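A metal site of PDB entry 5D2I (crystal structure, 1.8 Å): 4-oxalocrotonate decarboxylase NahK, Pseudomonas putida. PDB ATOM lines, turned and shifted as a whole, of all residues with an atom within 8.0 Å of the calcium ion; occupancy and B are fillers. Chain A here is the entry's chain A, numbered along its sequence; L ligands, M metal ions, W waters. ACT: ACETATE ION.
The calcium ion is bound by OE2 of Glu 116 (2.2 Å), OE1 of Glu 147 (2.2 Å), OE1 of Glu 114 (2.3 Å), water W2 (2.4 Å), O of the ligand (2.4 Å) and water W1 (2.4 Å).
The calcium ion has six donor atoms within binding distance.
N of Gly 240 is in hydrogen-bond range of OE1 of Glu 116 (2.9 Å).
The backbone NH (N) of Glu 116 sits at hydrogen-bond distance from the backbone carbonyl oxygen (O) of Thr 145.
OE2 of Glu 147 is in salt-bridge range of NZ of Lys 69, at 2.7 Å.
NZ of Lys 69 is in hydrogen-bond range of O of Ala 168 (2.8 Å).
NZ of Lys 69 sits close to OG of Ser 170 (3.2 Å).
Water W2 bridges the backbone NH (N) of Gly 241 (2.9 Å) and the backbone carbonyl oxygen (O) of Met 70 (3.2 Å).
Water W1 bridges O of Met 70 and OE1 of Glu 116.
Merely in contact with the calcium ion: Lys 69 (3.97 Å).
Of the 27 residues printed, 4 come within 4 Å of the calcium ion.
The nearest printed residue that does not touch the calcium ion is Met 70 (4.01 Å).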
ATOM      1  N   LYS A  69     -21.876  21.279  15.746  1.00  0.00           N
ATOM      2  CA  LYS A  69     -20.978  20.399  16.463  1.00  0.00           C
ATOM      3  C   LYS A  69     -20.380  19.421  15.484  1.00  0.00           C
ATOM      4  O   LYS A  69     -20.935  19.161  14.414  1.00  0.00           O
ATOM      5  CB  LYS A  69     -21.670  19.674  17.631  1.00  0.00           C
ATOM      6  CG  LYS A  69     -23.034  19.035  17.311  1.00  0.00           C
ATOM      7  CD  LYS A  69     -22.920  17.679  16.617  1.00  0.00           C
ATOM      8  CE  LYS A  69     -22.127  16.676  17.432  1.00  0.00           C
ATOM      9  NZ  LYS A  69     -22.963  16.016  18.494  1.00  0.00           N
ATOM     10  N   MET A  70     -19.219  18.895  15.852  1.00  0.00           N
ATOM     11  CA  MET A  70     -18.520  17.922  15.015  1.00  0.00           C
ATOM     12  C   MET A  70     -18.423  16.608  15.745  1.00  0.00           C
ATOM     13  O   MET A  70     -18.100  16.555  16.929  1.00  0.00           O
ATOM     14  CB  MET A  70     -17.122  18.429  14.672  1.00  0.00           C
ATOM     15  CG  MET A  70     -17.155  19.580  13.682  1.00  0.00           C
ATOM     16  SD  MET A  70     -17.602  19.001  12.054  1.00  0.00           S
ATOM     17  CE  MET A  70     -16.043  18.325  11.504  1.00  0.00           C
ATOM     18  N   GLY A  71     -18.724  15.534  15.017  1.00  0.00           N
ATOM     19  CA  GLY A  71     -18.652  14.198  15.569  1.00  0.00           C
ATOM     20  C   GLY A  71     -17.702  13.354  14.744  1.00  0.00           C
ATOM     21  O   GLY A  71     -17.323  13.761  13.635  1.00  0.00           O
ATOM     22  N   LEU A  72     -17.317  12.185  15.267  1.00  0.00           N
ATOM     23  CA  LEU A  72     -16.357  11.322  14.595  1.00  0.00           C
ATOM     24  C   LEU A  72     -15.093  12.109  14.281  1.00  0.00           C
ATOM     25  O   LEU A  72     -14.583  12.072  13.154  1.00  0.00           O
ATOM     26  CB  LEU A  72     -16.932  10.754  13.298  1.00  0.00           C
ATOM     27  CG  LEU A  72     -17.886   9.573  13.404  1.00  0.00           C
ATOM     28  CD1 LEU A  72     -18.304   9.153  12.002  1.00  0.00           C
ATOM     29  CD2 LEU A  72     -17.235   8.412  14.151  1.00  0.00           C
ATOM     30  N   THR A  73     -14.588  12.819  15.277  1.00  0.00           N
ATOM     31  CA  THR A  73     -13.421  13.674  15.084  1.00  0.00           C
ATOM     32  C   THR A  73     -12.183  12.937  15.573  1.00  0.00           C
ATOM     33  O   THR A  73     -11.252  13.536  16.108  1.00  0.00           O
ATOM     34  CB  THR A  73     -13.584  14.997  15.830  1.00  0.00           C
ATOM     35  OG1 THR A  73     -13.886  14.748  17.206  1.00  0.00           O
ATOM     36  CG2 THR A  73     -14.723  15.797  15.227  1.00  0.00           C
ATOM     37  N   LEU A  91     -26.730  22.807  16.644  1.00  0.00           N
ATOM     38  CA  LEU A  91     -27.135  22.982  18.026  1.00  0.00           C
ATOM     39  C   LEU A  91     -28.289  23.967  18.043  1.00  0.00           C
ATOM     40  O   LEU A  91     -28.188  25.062  17.491  1.00  0.00           O
ATOM     41  CB  LEU A  91     -25.975  23.537  18.845  1.00  0.00           C
ATOM     42  CG  LEU A  91     -24.698  22.695  18.781  1.00  0.00           C
ATOM     43  CD1 LEU A  91     -23.561  23.458  19.457  1.00  0.00           C
ATOM     44  CD2 LEU A  91     -24.926  21.328  19.455  1.00  0.00           C
ATOM     45  N   LYS A 112     -24.827  10.802  27.353  1.00  0.00           N
ATOM     46  CA  LYS A 112     -23.442  10.774  27.778  1.00  0.00           C
ATOM     47  C   LYS A 112     -22.887  12.163  27.608  1.00  0.00           C
ATOM     48  O   LYS A 112     -23.441  12.977  26.864  1.00  0.00           O
ATOM     49  CB  LYS A 112     -22.648   9.819  26.901  1.00  0.00           C
ATOM     50  CG  LYS A 112     -23.162   8.401  26.971  1.00  0.00           C
ATOM     51  CD  LYS A 112     -22.267   7.476  26.167  1.00  0.00           C
ATOM     52  CE  LYS A 112     -22.831   6.064  26.142  1.00  0.00           C
ATOM     53  NZ  LYS A 112     -21.929   5.135  25.425  1.00  0.00           N
ATOM     54  N   ILE A 113     -21.788  12.450  28.286  1.00  0.00           N
ATOM     55  CA  ILE A 113     -21.165  13.747  28.111  1.00  0.00           C
ATOM     56  C   ILE A 113     -19.782  13.580  27.501  1.00  0.00           C
ATOM     57  O   ILE A 113     -19.127  12.544  27.660  1.00  0.00           O
ATOM     58  CB  ILE A 113     -21.075  14.531  29.433  1.00  0.00           C
ATOM     59  CG1 ILE A 113     -20.276  13.749  30.474  1.00  0.00           C
ATOM     60  CG2 ILE A 113     -22.474  14.826  29.953  1.00  0.00           C
ATOM     61  CD1 ILE A 113     -19.925  14.581  31.714  1.00  0.00           C
ATOM     62  N   GLU A 114     -19.361  14.616  26.791  1.00  0.00           N
ATOM     63  CA  GLU A 114     -18.053  14.650  26.178  1.00  0.00           C
ATOM     64  C   GLU A 114     -17.490  16.017  26.455  1.00  0.00           C
ATOM     65  O   GLU A 114     -18.187  17.019  26.288  1.00  0.00           O
ATOM     66  CB  GLU A 114     -18.184  14.508  24.659  1.00  0.00           C
ATOM     67  CG  GLU A 114     -18.858  13.248  24.218  1.00  0.00           C
ATOM     68  CD  GLU A 114     -18.848  13.115  22.723  1.00  0.00           C
ATOM     69  OE1 GLU A 114     -19.438  13.985  22.042  1.00  0.00           O
ATOM     70  OE2 GLU A 114     -18.223  12.159  22.246  1.00  0.00           O
ATOM     71  N   ALA A 115     -16.225  16.063  26.860  1.00  0.00           N
ATOM     72  CA  ALA A 115     -15.533  17.334  27.050  1.00  0.00           C
ATOM     73  C   ALA A 115     -15.058  17.787  25.694  1.00  0.00           C
ATOM     74  O   ALA A 115     -14.444  17.015  24.958  1.00  0.00           O
ATOM     75  CB  ALA A 115     -14.358  17.142  27.962  1.00  0.00           C
ATOM     76  N   GLU A 116     -15.362  19.026  25.346  1.00  0.00           N
ATOM     77  CA  GLU A 116     -14.963  19.573  24.057  1.00  0.00           C
ATOM     78  C   GLU A 116     -14.440  20.971  24.215  1.00  0.00           C
ATOM     79  O   GLU A 116     -14.650  21.625  25.234  1.00  0.00           O
ATOM     80  CB  GLU A 116     -16.158  19.579  23.096  1.00  0.00           C
ATOM     81  CG  GLU A 116     -16.880  18.258  23.092  1.00  0.00           C
ATOM     82  CD  GLU A 116     -17.634  17.965  21.837  1.00  0.00           C
ATOM     83  OE1 GLU A 116     -17.526  18.716  20.841  1.00  0.00           O
ATOM     84  OE2 GLU A 116     -18.343  16.935  21.833  1.00  0.00           O
ATOM     85  N   THR A 145     -16.566  23.508  26.442  1.00  0.00           N
ATOM     86  CA  THR A 145     -17.939  23.074  26.256  1.00  0.00           C
ATOM     87  C   THR A 145     -18.045  21.590  26.500  1.00  0.00           C
ATOM     88  O   THR A 145     -17.252  20.822  25.994  1.00  0.00           O
ATOM     89  CB  THR A 145     -18.399  23.334  24.835  1.00  0.00           C
ATOM     90  OG1 THR A 145     -18.144  24.699  24.513  1.00  0.00           O
ATOM     91  CG2 THR A 145     -19.909  23.057  24.721  1.00  0.00           C
ATOM     92  N   VAL A 146     -19.047  21.207  27.281  1.00  0.00           N
ATOM     93  CA  VAL A 146     -19.315  19.798  27.497  1.00  0.00           C
ATOM     94  C   VAL A 146     -20.580  19.459  26.718  1.00  0.00           C
ATOM     95  O   VAL A 146     -21.628  20.060  26.939  1.00  0.00           O
ATOM     96  CB  VAL A 146     -19.516  19.512  28.973  1.00  0.00           C
ATOM     97  CG1 VAL A 146     -19.953  18.077  29.177  1.00  0.00           C
ATOM     98  CG2 VAL A 146     -18.222  19.782  29.723  1.00  0.00           C
ATOM     99  N   GLU A 147     -20.481  18.508  25.800  1.00  0.00           N
ATOM    100  CA  GLU A 147     -21.678  18.135  25.084  1.00  0.00           C
ATOM    101  C   GLU A 147     -22.385  17.074  25.854  1.00  0.00           C
ATOM    102  O   GLU A 147     -21.755  16.218  26.475  1.00  0.00           O
ATOM    103  CB  GLU A 147     -21.402  17.595  23.670  1.00  0.00           C
ATOM    104  CG  GLU A 147     -22.687  17.632  22.852  1.00  0.00           C
ATOM    105  CD  GLU A 147     -22.509  17.257  21.408  1.00  0.00           C
ATOM    106  OE1 GLU A 147     -21.457  16.703  21.040  1.00  0.00           O
ATOM    107  OE2 GLU A 147     -23.458  17.516  20.624  1.00  0.00           O
ATOM    108  N   VAL A 148     -23.711  17.140  25.861  1.00  0.00           N
ATOM    109  CA  VAL A 148     -24.482  15.980  26.247  1.00  0.00           C
ATOM    110  C   VAL A 148     -24.976  15.385  24.950  1.00  0.00           C
ATOM    111  O   VAL A 148     -25.724  16.036  24.214  1.00  0.00           O
ATOM    112  CB  VAL A 148     -25.671  16.337  27.115  1.00  0.00           C
ATOM    113  CG1 VAL A 148     -26.376  15.062  27.574  1.00  0.00           C
ATOM    114  CG2 VAL A 148     -25.189  17.130  28.326  1.00  0.00           C
ATOM    115  N   ILE A 149     -24.525  14.181  24.633  1.00  0.00           N
ATOM    116  CA  ILE A 149     -25.018  13.505  23.441  1.00  0.00           C
ATOM    117  C   ILE A 149     -26.015  12.469  23.859  1.00  0.00           C
ATOM    118  O   ILE A 149     -25.933  11.909  24.944  1.00  0.00           O
ATOM    119  CB  ILE A 149     -23.902  12.835  22.643  1.00  0.00           C
ATOM    120  CG1 ILE A 149     -22.994  12.026  23.564  1.00  0.00           C
ATOM    121  CG2 ILE A 149     -23.080  13.889  21.916  1.00  0.00           C
ATOM    122  CD1 ILE A 149     -21.965  11.224  22.794  1.00  0.00           C
ATOM    123  N   ALA A 168     -26.478  14.008  14.631  1.00  0.00           N
ATOM    124  CA  ALA A 168     -25.239  13.610  15.315  1.00  0.00           C
ATOM    125  C   ALA A 168     -25.438  13.506  16.818  1.00  0.00           C
ATOM    126  O   ALA A 168     -24.550  13.857  17.589  1.00  0.00           O
ATOM    127  CB  ALA A 168     -24.075  14.565  14.980  1.00  0.00           C
ATOM    128  N   SER A 169     -26.607  13.003  17.201  1.00  0.00           N
ATOM    129  CA  SER A 169     -26.935  12.702  18.596  1.00  0.00           C
ATOM    130  C   SER A 169     -26.913  13.931  19.495  1.00  0.00           C
ATOM    131  O   SER A 169     -26.790  13.807  20.714  1.00  0.00           O
ATOM    132  CB  SER A 169     -25.964  11.658  19.170  1.00  0.00           C
ATOM    133  OG  SER A 169     -25.810  10.560  18.300  1.00  0.00           O
ATOM    134  N   SER A 170     -27.067  15.112  18.916  1.00  0.00           N
ATOM    135  CA  SER A 170     -27.002  16.342  19.686  1.00  0.00           C
ATOM    136  C   SER A 170     -28.214  16.467  20.579  1.00  0.00           C
ATOM    137  O   SER A 170     -29.312  16.079  20.189  1.00  0.00           O
ATOM    138  CB  SER A 170     -26.926  17.554  18.763  1.00  0.00           C
ATOM    139  OG  SER A 170     -25.771  17.467  17.965  1.00  0.00           O
ATOM    140  N   ARG A 172     -27.777  18.466  24.257  1.00  0.00           N
ATOM    141  CA  ARG A 172     -27.451  19.581  25.125  1.00  0.00           C
ATOM    142  C   ARG A 172     -25.988  19.905  24.957  1.00  0.00           C
ATOM    143  O   ARG A 172     -25.180  19.060  24.558  1.00  0.00           O
ATOM    144  CB  ARG A 172     -27.703  19.267  26.600  1.00  0.00           C
ATOM    145  CG  ARG A 172     -29.110  18.825  26.935  1.00  0.00           C
ATOM    146  CD  ARG A 172     -30.087  19.973  26.962  1.00  0.00           C
ATOM    147  NE  ARG A 172     -31.393  19.493  27.399  1.00  0.00           N
ATOM    148  CZ  ARG A 172     -32.345  19.034  26.592  1.00  0.00           C
ATOM    149  NH1 ARG A 172     -32.160  19.032  25.273  1.00  0.00           N
ATOM    150  NH2 ARG A 172     -33.483  18.589  27.092  1.00  0.00           N
ATOM    151  N   MET A 238     -18.644  23.341  18.200  1.00  0.00           N
ATOM    152  CA  MET A 238     -18.064  22.398  19.149  1.00  0.00           C
ATOM    153  C   MET A 238     -17.227  21.448  18.332  1.00  0.00           C
ATOM    154  O   MET A 238     -17.741  20.758  17.434  1.00  0.00           O
ATOM    155  CB  MET A 238     -19.161  21.638  19.876  1.00  0.00           C
ATOM    156  CG  MET A 238     -20.075  22.543  20.628  1.00  0.00           C
ATOM    157  SD  MET A 238     -21.310  21.572  21.510  1.00  0.00           S
ATOM    158  CE  MET A 238     -20.244  20.463  22.371  1.00  0.00           C
ATOM    159  N   THR A 239     -15.933  21.410  18.616  1.00  0.00           N
ATOM    160  CA  THR A 239     -15.007  20.801  17.662  1.00  0.00           C
ATOM    161  C   THR A 239     -14.862  19.290  17.833  1.00  0.00           C
ATOM    162  O   THR A 239     -14.290  18.645  16.972  1.00  0.00           O
ATOM    163  CB  THR A 239     -13.632  21.461  17.695  1.00  0.00           C
ATOM    164  OG1 THR A 239     -13.083  21.331  19.003  1.00  0.00           O
ATOM    165  CG2 THR A 239     -13.756  22.942  17.337  1.00  0.00           C
ATOM    166  N   GLY A 240     -15.395  18.726  18.913  1.00  0.00           N
ATOM    167  CA  GLY A 240     -15.389  17.269  19.013  1.00  0.00           C
ATOM    168  C   GLY A 240     -14.993  16.743  20.376  1.00  0.00           C
ATOM    169  O   GLY A 240     -14.358  17.436  21.169  1.00  0.00           O
ATOM    170  N   GLY A 241     -15.358  15.486  20.640  1.00  0.00           N
ATOM    171  CA  GLY A 241     -15.058  14.880  21.934  1.00  0.00           C
ATOM    172  C   GLY A 241     -13.563  14.716  22.151  1.00  0.00           C
ATOM    173  O   GLY A 241     -12.864  14.051  21.381  1.00  0.00           O
ATOM    174  N   ILE A 242     -13.082  15.311  23.236  1.00  0.00           N
ATOM    175  CA  ILE A 242     -11.670  15.208  23.590  1.00  0.00           C
ATOM    176  C   ILE A 242     -11.485  13.947  24.405  1.00  0.00           C
ATOM    177  O   ILE A 242     -10.480  13.243  24.278  1.00  0.00           O
ATOM    178  CB  ILE A 242     -11.231  16.433  24.387  1.00  0.00           C
ATOM    179  CG1 ILE A 242     -11.210  17.654  23.462  1.00  0.00           C
ATOM    180  CG2 ILE A 242      -9.850  16.197  25.002  1.00  0.00           C
ATOM    181  CD1 ILE A 242     -10.919  18.972  24.176  1.00  0.00           C
ATOM    182  N   THR A 243     -12.473  13.659  25.237  1.00  0.00           N
ATOM    183  CA  THR A 243     -12.502  12.459  26.040  1.00  0.00           C
ATOM    184  C   THR A 243     -13.457  11.447  25.430  1.00  0.00           C
ATOM    185  O   THR A 243     -14.305  11.806  24.628  1.00  0.00           O
ATOM    186  CB  THR A 243     -13.007  12.784  27.438  1.00  0.00           C
ATOM    187  OG1 THR A 243     -14.317  13.374  27.341  1.00  0.00           O
ATOM    188  CG2 THR A 243     -12.078  13.786  28.108  1.00  0.00           C
ATOM    189  N   ALA A 245     -16.782   9.394  25.696  1.00  0.00           N
ATOM    190  CA  ALA A 245     -18.054   9.918  26.201  1.00  0.00           C
ATOM    191  C   ALA A 245     -18.371   9.189  27.500  1.00  0.00           C
ATOM    192  O   ALA A 245     -18.081   8.012  27.640  1.00  0.00           O
ATOM    193  CB  ALA A 245     -19.168   9.721  25.181  1.00  0.00           C
HETATM  194  C   ACT L   1     -20.574  13.151  18.562  1.00  0.00           C
HETATM  195  O   ACT L   1     -20.746  14.286  19.042  1.00  0.00           O
HETATM  196  OXT ACT L   1     -19.385  12.758  18.501  1.00  0.00           O
HETATM  197  CH3 ACT L   1     -21.725  12.321  18.100  1.00  0.00           C
HETATM  198 CA    CA M   1     -19.582  15.693  20.550  1.00  0.00          CA
HETATM  199  O   HOH W   1     -19.171  17.476  19.045  1.00  0.00           O
HETATM  200  O   HOH W   2     -17.853  14.568  19.393  1.00  0.00           O
